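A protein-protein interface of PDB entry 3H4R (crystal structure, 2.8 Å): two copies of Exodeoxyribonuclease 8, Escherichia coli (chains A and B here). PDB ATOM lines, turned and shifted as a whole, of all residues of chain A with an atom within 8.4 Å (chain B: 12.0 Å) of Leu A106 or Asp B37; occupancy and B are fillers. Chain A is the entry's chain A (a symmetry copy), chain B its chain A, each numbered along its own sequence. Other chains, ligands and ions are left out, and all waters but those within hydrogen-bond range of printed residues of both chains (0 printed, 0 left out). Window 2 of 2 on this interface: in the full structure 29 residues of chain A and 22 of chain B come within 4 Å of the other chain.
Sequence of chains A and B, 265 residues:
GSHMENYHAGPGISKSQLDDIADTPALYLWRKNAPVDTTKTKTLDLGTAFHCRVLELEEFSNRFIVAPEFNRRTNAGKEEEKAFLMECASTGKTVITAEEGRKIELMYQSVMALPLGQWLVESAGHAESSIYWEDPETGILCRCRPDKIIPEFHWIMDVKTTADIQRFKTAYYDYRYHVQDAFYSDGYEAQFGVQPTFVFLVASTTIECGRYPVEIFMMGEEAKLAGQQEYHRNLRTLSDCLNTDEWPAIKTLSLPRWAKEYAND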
ATOM      1  N   PHE A  50      20.911  15.586 -27.505  1.00  0.00           N
ATOM      2  CA  PHE A  50      20.484  14.939 -26.277  1.00  0.00           C
ATOM      3  C   PHE A  50      21.478  13.832 -25.956  1.00  0.00           C
ATOM      4  O   PHE A  50      21.976  13.720 -24.833  1.00  0.00           O
ATOM      5  CB  PHE A  50      19.093  14.340 -26.461  1.00  0.00           C
ATOM      6  CG  PHE A  50      18.546  13.709 -25.221  1.00  0.00           C
ATOM      7  CD1 PHE A  50      18.289  14.476 -24.096  1.00  0.00           C
ATOM      8  CD2 PHE A  50      18.317  12.346 -25.162  1.00  0.00           C
ATOM      9  CE1 PHE A  50      17.811  13.890 -22.933  1.00  0.00           C
ATOM     10  CE2 PHE A  50      17.840  11.756 -24.002  1.00  0.00           C
ATOM     11  CZ  PHE A  50      17.589  12.529 -22.888  1.00  0.00           C
ATOM     12  N   ARG A  53      24.304  15.304 -24.411  1.00  0.00           N
ATOM     13  CA  ARG A  53      23.989  15.902 -23.117  1.00  0.00           C
ATOM     14  C   ARG A  53      24.057  14.799 -22.072  1.00  0.00           C
ATOM     15  O   ARG A  53      24.831  14.869 -21.126  1.00  0.00           O
ATOM     16  CB  ARG A  53      22.578  16.516 -23.128  1.00  0.00           C
ATOM     17  CG  ARG A  53      22.298  17.588 -22.052  1.00  0.00           C
ATOM     18  CD  ARG A  53      22.894  17.230 -20.700  1.00  0.00           C
ATOM     19  NE  ARG A  53      22.419  18.090 -19.620  1.00  0.00           N
ATOM     20  CZ  ARG A  53      22.834  18.000 -18.356  1.00  0.00           C
ATOM     21  NH1 ARG A  53      23.738  17.091 -18.008  1.00  0.00           N
ATOM     22  NH2 ARG A  53      22.329  18.799 -17.426  1.00  0.00           N
ATOM     23  N   GLU A  99      16.006  28.393 -29.136  1.00  0.00           N
ATOM     24  CA  GLU A  99      15.038  28.489 -28.032  1.00  0.00           C
ATOM     25  C   GLU A  99      14.589  27.062 -27.712  1.00  0.00           C
ATOM     26  O   GLU A  99      13.580  26.831 -27.032  1.00  0.00           O
ATOM     27  CB  GLU A  99      13.837  29.343 -28.452  1.00  0.00           C
ATOM     28  N   GLU A 100      15.371  26.116 -28.235  1.00  0.00           N
ATOM     29  CA  GLU A 100      15.152  24.684 -28.077  1.00  0.00           C
ATOM     30  C   GLU A 100      16.144  24.134 -27.054  1.00  0.00           C
ATOM     31  O   GLU A 100      15.906  23.089 -26.447  1.00  0.00           O
ATOM     32  CB  GLU A 100      15.346  23.985 -29.423  1.00  0.00           C
ATOM     33  N   GLY A 101      17.255  24.845 -26.870  1.00  0.00           N
ATOM     34  CA  GLY A 101      18.271  24.427 -25.917  1.00  0.00           C
ATOM     35  C   GLY A 101      17.705  24.266 -24.520  1.00  0.00           C
ATOM     36  O   GLY A 101      18.401  23.821 -23.600  1.00  0.00           O
ATOM     37  N   ARG A 102      16.438  24.646 -24.364  1.00  0.00           N
ATOM     38  CA  ARG A 102      15.747  24.534 -23.085  1.00  0.00           C
ATOM     39  C   ARG A 102      15.104  23.149 -22.977  1.00  0.00           C
ATOM     40  O   ARG A 102      15.076  22.553 -21.893  1.00  0.00           O
ATOM     41  CB  ARG A 102      14.672  25.623 -22.947  1.00  0.00           C
ATOM     42  CG  ARG A 102      13.463  25.480 -23.875  1.00  0.00           C
ATOM     43  CD  ARG A 102      12.341  26.406 -23.417  1.00  0.00           C
ATOM     44  NE  ARG A 102      11.901  26.086 -22.058  1.00  0.00           N
ATOM     45  CZ  ARG A 102      11.257  26.928 -21.253  1.00  0.00           C
ATOM     46  NH1 ARG A 102      10.974  28.160 -21.664  1.00  0.00           N
ATOM     47  NH2 ARG A 102      10.898  26.537 -20.036  1.00  0.00           N
ATOM     48  N   LYS A 103      14.587  22.643 -24.100  1.00  0.00           N
ATOM     49  CA  LYS A 103      13.971  21.318 -24.126  1.00  0.00           C
ATOM     50  C   LYS A 103      15.032  20.322 -23.675  1.00  0.00           C
ATOM     51  O   LYS A 103      14.833  19.596 -22.703  1.00  0.00           O
ATOM     52  CB  LYS A 103      13.492  20.972 -25.532  1.00  0.00           C
ATOM     53  N   ILE A 104      16.167  20.313 -24.373  1.00  0.00           N
ATOM     54  CA  ILE A 104      17.275  19.415 -24.056  1.00  0.00           C
ATOM     55  C   ILE A 104      17.619  19.407 -22.571  1.00  0.00           C
ATOM     56  O   ILE A 104      18.019  18.380 -22.016  1.00  0.00           O
ATOM     57  CB  ILE A 104      18.539  19.786 -24.860  1.00  0.00           C
ATOM     58  CG1 ILE A 104      18.313  19.467 -26.341  1.00  0.00           C
ATOM     59  CG2 ILE A 104      19.749  19.050 -24.304  1.00  0.00           C
ATOM     60  CD1 ILE A 104      19.555  19.528 -27.202  1.00  0.00           C
ATOM     61  N   GLU A 105      17.468  20.552 -21.923  1.00  0.00           N
ATOM     62  CA  GLU A 105      17.767  20.629 -20.507  1.00  0.00           C
ATOM     63  C   GLU A 105      16.593  20.059 -19.716  1.00  0.00           C
ATOM     64  O   GLU A 105      16.779  19.453 -18.656  1.00  0.00           O
ATOM     65  CB  GLU A 105      18.050  22.075 -20.103  1.00  0.00           C
ATOM     66  CG  GLU A 105      18.530  22.212 -18.670  1.00  0.00           C
ATOM     67  CD  GLU A 105      19.427  21.059 -18.256  1.00  0.00           C
ATOM     68  OE1 GLU A 105      20.377  20.752 -19.018  1.00  0.00           O
ATOM     69  OE2 GLU A 105      19.180  20.467 -17.172  1.00  0.00           O
ATOM     70  N   LEU A 106      15.387  20.249 -20.242  1.00  0.00           N
ATOM     71  CA  LEU A 106      14.180  19.734 -19.604  1.00  0.00           C
ATOM     72  C   LEU A 106      14.101  18.208 -19.746  1.00  0.00           C
ATOM     73  O   LEU A 106      13.807  17.498 -18.776  1.00  0.00           O
ATOM     74  CB  LEU A 106      12.945  20.389 -20.219  1.00  0.00           C
ATOM     75  CG  LEU A 106      12.509  21.671 -19.513  1.00  0.00           C
ATOM     76  CD1 LEU A 106      11.410  22.377 -20.295  1.00  0.00           C
ATOM     77  CD2 LEU A 106      12.028  21.304 -18.120  1.00  0.00           C
ATOM     78  N   MET A 107      14.358  17.708 -20.957  1.00  0.00           N
ATOM     79  CA  MET A 107      14.345  16.270 -21.218  1.00  0.00           C
ATOM     80  C   MET A 107      15.322  15.626 -20.253  1.00  0.00           C
ATOM     81  O   MET A 107      14.927  14.823 -19.417  1.00  0.00           O
ATOM     82  CB  MET A 107      14.786  15.961 -22.651  1.00  0.00           C
ATOM     83  CG  MET A 107      13.760  16.269 -23.716  1.00  0.00           C
ATOM     84  SD  MET A 107      14.434  16.034 -25.375  1.00  0.00           S
ATOM     85  CE  MET A 107      13.923  14.382 -25.702  1.00  0.00           C
ATOM     86  N   TYR A 108      16.596  15.994 -20.359  1.00  0.00           N
ATOM     87  CA  TYR A 108      17.607  15.432 -19.478  1.00  0.00           C
ATOM     88  C   TYR A 108      17.160  15.418 -18.027  1.00  0.00           C
ATOM     89  O   TYR A 108      17.506  14.507 -17.274  1.00  0.00           O
ATOM     90  CB  TYR A 108      18.923  16.200 -19.577  1.00  0.00           C
ATOM     91  CG  TYR A 108      19.963  15.696 -18.597  1.00  0.00           C
ATOM     92  CD1 TYR A 108      19.892  16.020 -17.240  1.00  0.00           C
ATOM     93  CD2 TYR A 108      21.014  14.887 -19.024  1.00  0.00           C
ATOM     94  CE1 TYR A 108      20.844  15.557 -16.332  1.00  0.00           C
ATOM     95  CE2 TYR A 108      21.977  14.418 -18.125  1.00  0.00           C
ATOM     96  CZ  TYR A 108      21.886  14.760 -16.782  1.00  0.00           C
ATOM     97  OH  TYR A 108      22.853  14.330 -15.900  1.00  0.00           O
ATOM     98  N   GLN A 109      16.401  16.428 -17.622  1.00  0.00           N
ATOM     99  CA  GLN A 109      15.944  16.485 -16.243  1.00  0.00           C
ATOM    100  C   GLN A 109      14.796  15.501 -16.018  1.00  0.00           C
ATOM    101  O   GLN A 109      14.477  15.139 -14.881  1.00  0.00           O
ATOM    102  CB  GLN A 109      15.524  17.916 -15.884  1.00  0.00           C
ATOM    103  CG  GLN A 109      15.386  18.137 -14.387  1.00  0.00           C
ATOM    104  CD  GLN A 109      16.539  17.520 -13.603  1.00  0.00           C
ATOM    105  OE1 GLN A 109      17.709  17.863 -13.811  1.00  0.00           O
ATOM    106  NE2 GLN A 109      16.213  16.605 -12.697  1.00  0.00           N
ATOM    107  N   SER A 110      14.196  15.052 -17.115  1.00  0.00           N
ATOM    108  CA  SER A 110      13.091  14.106 -17.054  1.00  0.00           C
ATOM    109  C   SER A 110      13.563  12.675 -16.814  1.00  0.00           C
ATOM    110  O   SER A 110      12.921  11.928 -16.075  1.00  0.00           O
ATOM    111  CB  SER A 110      12.277  14.163 -18.345  1.00  0.00           C
ATOM    112  OG  SER A 110      11.220  13.223 -18.300  1.00  0.00           O
ATOM    113  N   VAL A 111      14.677  12.290 -17.438  1.00  0.00           N
ATOM    114  CA  VAL A 111      15.207  10.940 -17.255  1.00  0.00           C
ATOM    115  C   VAL A 111      15.851  10.822 -15.872  1.00  0.00           C
ATOM    116  O   VAL A 111      16.024   9.724 -15.354  1.00  0.00           O
ATOM    117  CB  VAL A 111      16.259  10.545 -18.357  1.00  0.00           C
ATOM    118  CG1 VAL A 111      15.879  11.155 -19.691  1.00  0.00           C
ATOM    119  CG2 VAL A 111      17.656  10.942 -17.939  1.00  0.00           C
ATOM    120  N   MET A 112      16.204  11.957 -15.276  1.00  0.00           N
ATOM    121  CA  MET A 112      16.808  11.949 -13.946  1.00  0.00           C
ATOM    122  C   MET A 112      15.710  11.672 -12.925  1.00  0.00           C
ATOM    123  O   MET A 112      15.979  11.327 -11.773  1.00  0.00           O
ATOM    124  CB  MET A 112      17.463  13.298 -13.641  1.00  0.00           C
ATOM    125  CG  MET A 112      18.570  13.712 -14.604  1.00  0.00           C
ATOM    126  SD  MET A 112      19.896  12.496 -14.793  1.00  0.00           S
ATOM    127  CE  MET A 112      20.276  12.099 -13.096  1.00  0.00           C
ATOM    128  N   ALA A 113      14.468  11.825 -13.366  1.00  0.00           N
ATOM    129  CA  ALA A 113      13.317  11.606 -12.509  1.00  0.00           C
ATOM    130  C   ALA A 113      13.142  10.132 -12.157  1.00  0.00           C
ATOM    131  O   ALA A 113      13.353   9.750 -11.003  1.00  0.00           O
ATOM    132  CB  ALA A 113      12.073  12.135 -13.179  1.00  0.00           C
ATOM    133  N   SER A 204      11.281  11.350 -25.426  1.00  0.00           N
ATOM    134  CA  SER A 204      10.489  11.976 -26.480  1.00  0.00           C
ATOM    135  C   SER A 204      10.748  13.459 -26.717  1.00  0.00           C
ATOM    136  O   SER A 204      10.908  14.245 -25.783  1.00  0.00           O
ATOM    137  CB  SER A 204       8.990  11.786 -26.220  1.00  0.00           C
ATOM    138  OG  SER A 204       8.537  12.603 -25.151  1.00  0.00           O
ATOM    139  N   ILE A 207       6.570  16.921 -26.208  1.00  0.00           N
ATOM    140  CA  ILE A 207       5.871  17.034 -24.933  1.00  0.00           C
ATOM    141  C   ILE A 207       4.472  16.450 -24.979  1.00  0.00           C
ATOM    142  O   ILE A 207       3.776  16.546 -25.986  1.00  0.00           O
ATOM    143  CB  ILE A 207       5.768  18.509 -24.491  1.00  0.00           C
ATOM    144  CG1 ILE A 207       5.067  18.601 -23.132  1.00  0.00           C
ATOM    145  CG2 ILE A 207       5.013  19.300 -25.540  1.00  0.00           C
ATOM    146  CD1 ILE A 207       5.095  19.987 -22.504  1.00  0.00           C
ATOM    147  N   CYS A 209       1.036  16.109 -22.287  1.00  0.00           N
ATOM    148  CA  CYS A 209       0.413  16.448 -21.016  1.00  0.00           C
ATOM    149  C   CYS A 209       1.346  17.218 -20.078  1.00  0.00           C
ATOM    150  O   CYS A 209       1.389  16.949 -18.876  1.00  0.00           O
ATOM    151  CB  CYS A 209      -0.083  15.167 -20.330  1.00  0.00           C
ATOM    152  SG  CYS A 209      -1.117  15.421 -18.862  1.00  0.00           S
ATOM    153  N   GLY A 210       2.108  18.157 -20.634  1.00  0.00           N
ATOM    154  CA  GLY A 210       2.986  18.972 -19.811  1.00  0.00           C
ATOM    155  C   GLY A 210       4.428  18.568 -19.573  1.00  0.00           C
ATOM    156  O   GLY A 210       5.224  19.381 -19.096  1.00  0.00           O
ATOM    157  N   ARG A 211       4.790  17.331 -19.887  1.00  0.00           N
ATOM    158  CA  ARG A 211       6.167  16.909 -19.671  1.00  0.00           C
ATOM    159  C   ARG A 211       6.726  16.198 -20.898  1.00  0.00           C
ATOM    160  O   ARG A 211       6.053  16.107 -21.926  1.00  0.00           O
ATOM    161  CB  ARG A 211       6.238  15.992 -18.453  1.00  0.00           C
ATOM    162  CG  ARG A 211       5.467  16.515 -17.249  1.00  0.00           C
ATOM    163  CD  ARG A 211       6.026  15.940 -15.956  1.00  0.00           C
ATOM    164  NE  ARG A 211       5.155  16.111 -14.791  1.00  0.00           N
ATOM    165  CZ  ARG A 211       3.930  15.604 -14.689  1.00  0.00           C
ATOM    166  NH1 ARG A 211       3.414  14.894 -15.690  1.00  0.00           N
ATOM    167  NH2 ARG A 211       3.229  15.784 -13.574  1.00  0.00           N
ATOM    168  N   TYR A 212       7.971  15.733 -20.799  1.00  0.00           N
ATOM    169  CA  TYR A 212       8.623  14.987 -21.884  1.00  0.00           C
ATOM    170  C   TYR A 212       8.904  13.605 -21.306  1.00  0.00           C
ATOM    171  O   TYR A 212       9.910  13.411 -20.625  1.00  0.00           O
ATOM    172  CB  TYR A 212       9.944  15.636 -22.293  1.00  0.00           C
ATOM    173  CG  TYR A 212       9.800  16.915 -23.075  1.00  0.00           C
ATOM    174  CD1 TYR A 212       9.110  16.944 -24.282  1.00  0.00           C
ATOM    175  CD2 TYR A 212      10.412  18.092 -22.637  1.00  0.00           C
ATOM    176  CE1 TYR A 212       9.038  18.120 -25.040  1.00  0.00           C
ATOM    177  CE2 TYR A 212      10.349  19.272 -23.387  1.00  0.00           C
ATOM    178  CZ  TYR A 212       9.665  19.276 -24.584  1.00  0.00           C
ATOM    179  OH  TYR A 212       9.637  20.422 -25.334  1.00  0.00           O
ATOM    180  N   PRO A 213       8.021  12.628 -21.576  1.00  0.00           N
ATOM    181  CA  PRO A 213       8.193  11.272 -21.055  1.00  0.00           C
ATOM    182  C   PRO A 213       9.455  10.539 -21.479  1.00  0.00           C
ATOM    183  O   PRO A 213       9.982  10.734 -22.578  1.00  0.00           O
ATOM    184  CB  PRO A 213       6.925  10.570 -21.524  1.00  0.00           C
ATOM    185  CG  PRO A 213       6.666  11.221 -22.835  1.00  0.00           C
ATOM    186  CD  PRO A 213       6.903  12.677 -22.536  1.00  0.00           C
ATOM    187  N   VAL A 214       9.933   9.701 -20.571  1.00  0.00           N
ATOM    188  CA  VAL A 214      11.111   8.884 -20.800  1.00  0.00           C
ATOM    189  C   VAL A 214      10.720   7.438 -20.486  1.00  0.00           C
ATOM    190  O   VAL A 214       9.824   7.190 -19.674  1.00  0.00           O
ATOM    191  CB  VAL A 214      12.279   9.311 -19.890  1.00  0.00           C
ATOM    192  CG1 VAL A 214      13.510   8.465 -20.195  1.00  0.00           C
ATOM    193  CG2 VAL A 214      12.598  10.772 -20.108  1.00  0.00           C
ATOM    194  N   TRP B  30       7.647   8.715 -11.077  1.00  0.00           N
ATOM    195  CA  TRP B  30       8.383   9.554 -12.023  1.00  0.00           C
ATOM    196  C   TRP B  30       7.584  10.855 -12.081  1.00  0.00           C
ATOM    197  O   TRP B  30       8.099  11.946 -11.802  1.00  0.00           O
ATOM    198  CB  TRP B  30       8.394   8.901 -13.417  1.00  0.00           C
ATOM    199  CG  TRP B  30       8.775   9.832 -14.546  1.00  0.00           C
ATOM    200  CD1 TRP B  30      10.027  10.286 -14.848  1.00  0.00           C
ATOM    201  CD2 TRP B  30       7.892  10.430 -15.509  1.00  0.00           C
ATOM    202  NE1 TRP B  30       9.983  11.129 -15.937  1.00  0.00           N
ATOM    203  CE2 TRP B  30       8.687  11.236 -16.363  1.00  0.00           C
ATOM    204  CE3 TRP B  30       6.509  10.366 -15.732  1.00  0.00           C
ATOM    205  CZ2 TRP B  30       8.146  11.972 -17.427  1.00  0.00           C
ATOM    206  CZ3 TRP B  30       5.968  11.103 -16.793  1.00  0.00           C
ATOM    207  CH2 TRP B  30       6.790  11.895 -17.626  1.00  0.00           C
ATOM    208  N   ARG B  31       6.313  10.695 -12.452  1.00  0.00           N
ATOM    209  CA  ARG B  31       5.319  11.764 -12.582  1.00  0.00           C
ATOM    210  C   ARG B  31       5.513  12.800 -11.487  1.00  0.00           C
ATOM    211  O   ARG B  31       5.598  14.014 -11.736  1.00  0.00           O
ATOM    212  CB  ARG B  31       3.926  11.145 -12.451  1.00  0.00           C
ATOM    213  CG  ARG B  31       2.768  12.053 -12.766  1.00  0.00           C
ATOM    214  CD  ARG B  31       2.023  11.527 -13.974  1.00  0.00           C
ATOM    215  NE  ARG B  31       2.601  12.011 -15.222  1.00  0.00           N
ATOM    216  CZ  ARG B  31       2.391  11.444 -16.405  1.00  0.00           C
ATOM    217  NH1 ARG B  31       1.621  10.364 -16.486  1.00  0.00           N
ATOM    218  NH2 ARG B  31       2.936  11.965 -17.501  1.00  0.00           N
ATOM    219  N   ASN B  33       7.819  14.067 -10.006  1.00  0.00           N
ATOM    220  CA  ASN B  33       9.207  14.538  -9.993  1.00  0.00           C
ATOM    221  C   ASN B  33       9.605  15.232 -11.293  1.00  0.00           C
ATOM    222  O   ASN B  33      10.215  16.307 -11.277  1.00  0.00           O
ATOM    223  CB  ASN B  33      10.187  13.387  -9.735  1.00  0.00           C
ATOM    224  CG  ASN B  33      10.450  13.163  -8.264  1.00  0.00           C
ATOM    225  OD1 ASN B  33      10.695  14.112  -7.521  1.00  0.00           O
ATOM    226  ND2 ASN B  33      10.409  11.905  -7.834  1.00  0.00           N
ATOM    227  N   ALA B  34       9.270  14.612 -12.418  1.00  0.00           N
ATOM    228  CA  ALA B  34       9.614  15.181 -13.712  1.00  0.00           C
ATOM    229  C   ALA B  34       9.081  16.600 -13.818  1.00  0.00           C
ATOM    230  O   ALA B  34       7.877  16.837 -13.731  1.00  0.00           O
ATOM    231  CB  ALA B  34       9.052  14.326 -14.832  1.00  0.00           C
ATOM    232  N   PRO B  35       9.983  17.568 -13.991  1.00  0.00           N
ATOM    233  CA  PRO B  35       9.583  18.968 -14.107  1.00  0.00           C
ATOM    234  C   PRO B  35       8.792  19.229 -15.391  1.00  0.00           C
ATOM    235  O   PRO B  35       9.079  18.637 -16.431  1.00  0.00           O
ATOM    236  CB  PRO B  35      10.923  19.699 -14.083  1.00  0.00           C
ATOM    237  CG  PRO B  35      11.844  18.718 -14.759  1.00  0.00           C
ATOM    238  CD  PRO B  35      11.446  17.426 -14.100  1.00  0.00           C
ATOM    239  N   VAL B  36       7.792  20.105 -15.306  1.00  0.00           N
ATOM    240  CA  VAL B  36       6.969  20.462 -16.460  1.00  0.00           C
ATOM    241  C   VAL B  36       7.519  21.763 -17.062  1.00  0.00           C
ATOM    242  O   VAL B  36       8.265  22.493 -16.397  1.00  0.00           O
ATOM    243  CB  VAL B  36       5.512  20.647 -16.025  1.00  0.00           C
ATOM    244  N   ASP B  37       7.168  22.045 -18.319  1.00  0.00           N
ATOM    245  CA  ASP B  37       7.620  23.270 -18.989  1.00  0.00           C
ATOM    246  C   ASP B  37       6.514  24.325 -18.932  1.00  0.00           C
ATOM    247  O   ASP B  37       5.855  24.594 -19.943  1.00  0.00           O
ATOM    248  CB  ASP B  37       7.992  22.980 -20.443  1.00  0.00           C
ATOM    249  N   THR B  38       6.322  24.907 -17.743  1.00  0.00           N
ATOM    250  CA  THR B  38       5.302  25.932 -17.495  1.00  0.00           C
ATOM    251  C   THR B  38       5.322  27.030 -18.558  1.00  0.00           C
ATOM    252  O   THR B  38       5.987  28.059 -18.399  1.00  0.00           O
ATOM    253  CB  THR B  38       5.499  26.539 -16.100  1.00  0.00           C
ATOM    254  N   THR B  39       4.581  26.792 -19.641  1.00  0.00           N
ATOM    255  CA  THR B  39       4.486  27.721 -20.764  1.00  0.00           C
ATOM    256  C   THR B  39       3.278  27.384 -21.646  1.00  0.00           C
ATOM    257  O   THR B  39       3.422  27.202 -22.857  1.00  0.00           O
ATOM    258  CB  THR B  39       5.779  27.674 -21.597  1.00  0.00           C
ATOM    259  N   LYS B  40       2.093  27.306 -21.030  1.00  0.00           N
ATOM    260  CA  LYS B  40       0.838  26.989 -21.731  1.00  0.00           C
ATOM    261  C   LYS B  40       0.566  27.935 -22.912  1.00  0.00           C
ATOM    262  O   LYS B  40      -0.132  28.943 -22.770  1.00  0.00           O
ATOM    263  CB  LYS B  40      -0.344  27.031 -20.740  1.00  0.00           C
ATOM    264  N   THR B  41       1.112  27.593 -24.078  1.00  0.00           N
ATOM    265  CA  THR B  41       0.951  28.409 -25.278  1.00  0.00           C
ATOM    266  C   THR B  41       0.184  27.695 -26.390  1.00  0.00           C
ATOM    267  O   THR B  41       0.787  27.031 -27.242  1.00  0.00           O
ATOM    268  CB  THR B  41       2.327  28.847 -25.791  1.00  0.00           C
ATOM    269  N   LYS B  42      -1.142  27.839 -26.379  1.00  0.00           N
ATOM    270  CA  LYS B  42      -1.997  27.220 -27.392  1.00  0.00           C
ATOM    271  C   LYS B  42      -3.490  27.465 -27.152  1.00  0.00           C
ATOM    272  O   LYS B  42      -4.274  27.528 -28.110  1.00  0.00           O
ATOM    273  CB  LYS B  42      -1.725  25.716 -27.461  1.00  0.00           C
ATOM    274  N   THR B  43      -3.878  27.602 -25.880  1.00  0.00           N
ATOM    275  CA  THR B  43      -5.281  27.819 -25.500  1.00  0.00           C
ATOM    276  C   THR B  43      -6.129  26.629 -25.972  1.00  0.00           C
ATOM    277  O   THR B  43      -7.361  26.658 -25.891  1.00  0.00           O
ATOM    278  CB  THR B  43      -5.810  29.131 -26.116  1.00  0.00           C
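Of the 13 printed residues of chain B, 6 touch a printed residue of chain A. Hydrophobic or aromatic side chains of chain B that line the printed part of chain A: Trp B30, Ala B34, Pro B35 and Val B36. Of the 25 printed residues of chain A, 8 touch a printed residue of chain B. Hydrophobic or aromatic side chains of chain A within 4 Å of the printed part of chain B: Leu A106 and Ala A113. Along chain A the printed residues that touch a printed residue of chain B span positions 106 to 213. Among the printed residues, no Asp or Glu carboxylate lies within 4 Å of a Lys or Arg side-chain nitrogen of the other chain.
OG of Ser A110 sits at hydrogen-bond distance from O of Tyr A212 (2.7 Å). O of Pro A213 sits at hydrogen-bond distance from N of Ser A204 (3.2 Å).
Among the printed residues, pairs that only touch across the chains: Leu A106 with Asp B37 (3.5 Å), Gln A109 with Pro B35 (3.6 Å), Ala A113 with Trp B30 (3.2 Å), Ala A113 with Ala B34 (3.8 Å), Gly A210 with Val B36 (3.3 Å), Tyr A212 with Trp B30 (3.9 Å) and Pro A213 with Trp B30 (3.7 Å).
No position is printed for both chains. Of the 11 pairs that touch across the chains among the printed residues, none has its exchanged pair printed and touching as well.
The guanidinium group (NH2) of Arg A211 sits at hydrogen-bond distance from the backbone carbonyl oxygen (O) of Arg B31 (3.5 Å). O of Ser A110 sits at hydrogen-bond distance from NE1 of Trp B30, at 3.0 Å. NE of Arg A211 sits at hydrogen-bond distance from O of Ala B34. N of Asp B37 is in hydrogen-bond range of O of Gly A210, 3.4 Å away.
Of chain B, only Asp B37 comes within 4 Å of Leu A106. Of chain A, only Leu A106 and Gly A210 come within 4 Å of Asp B37. No residue of chain B comes within 4 Å of Arg A102. No residue of chain B comes within 4 Å of Met A107. Gly A210 touches just these residues of chain B: Val B36 and Asp B37. Of chain B, only Trp B30 (3.9 Å) comes within 4 Å of Tyr A212. Of the printed residues of chain A, Arg B31 touches Arg A211. Of the printed residues of chain A, Ala B34 touches Ala A113 (3.8 Å) and Arg A211 (3.0 Å). Of the printed residues of chain A, Trp B30 touches Ser A110, Ala A113, Tyr A212 and Pro A213. Of the printed residues of chain B, Arg A211 touches Arg B31 and Ala B34. Of the printed residues of chain B, Pro A213 touches Trp B30 (3.7 Å). The nearest residue of chain A that does not touch Asp B37 is Arg A102 (4.6 Å).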
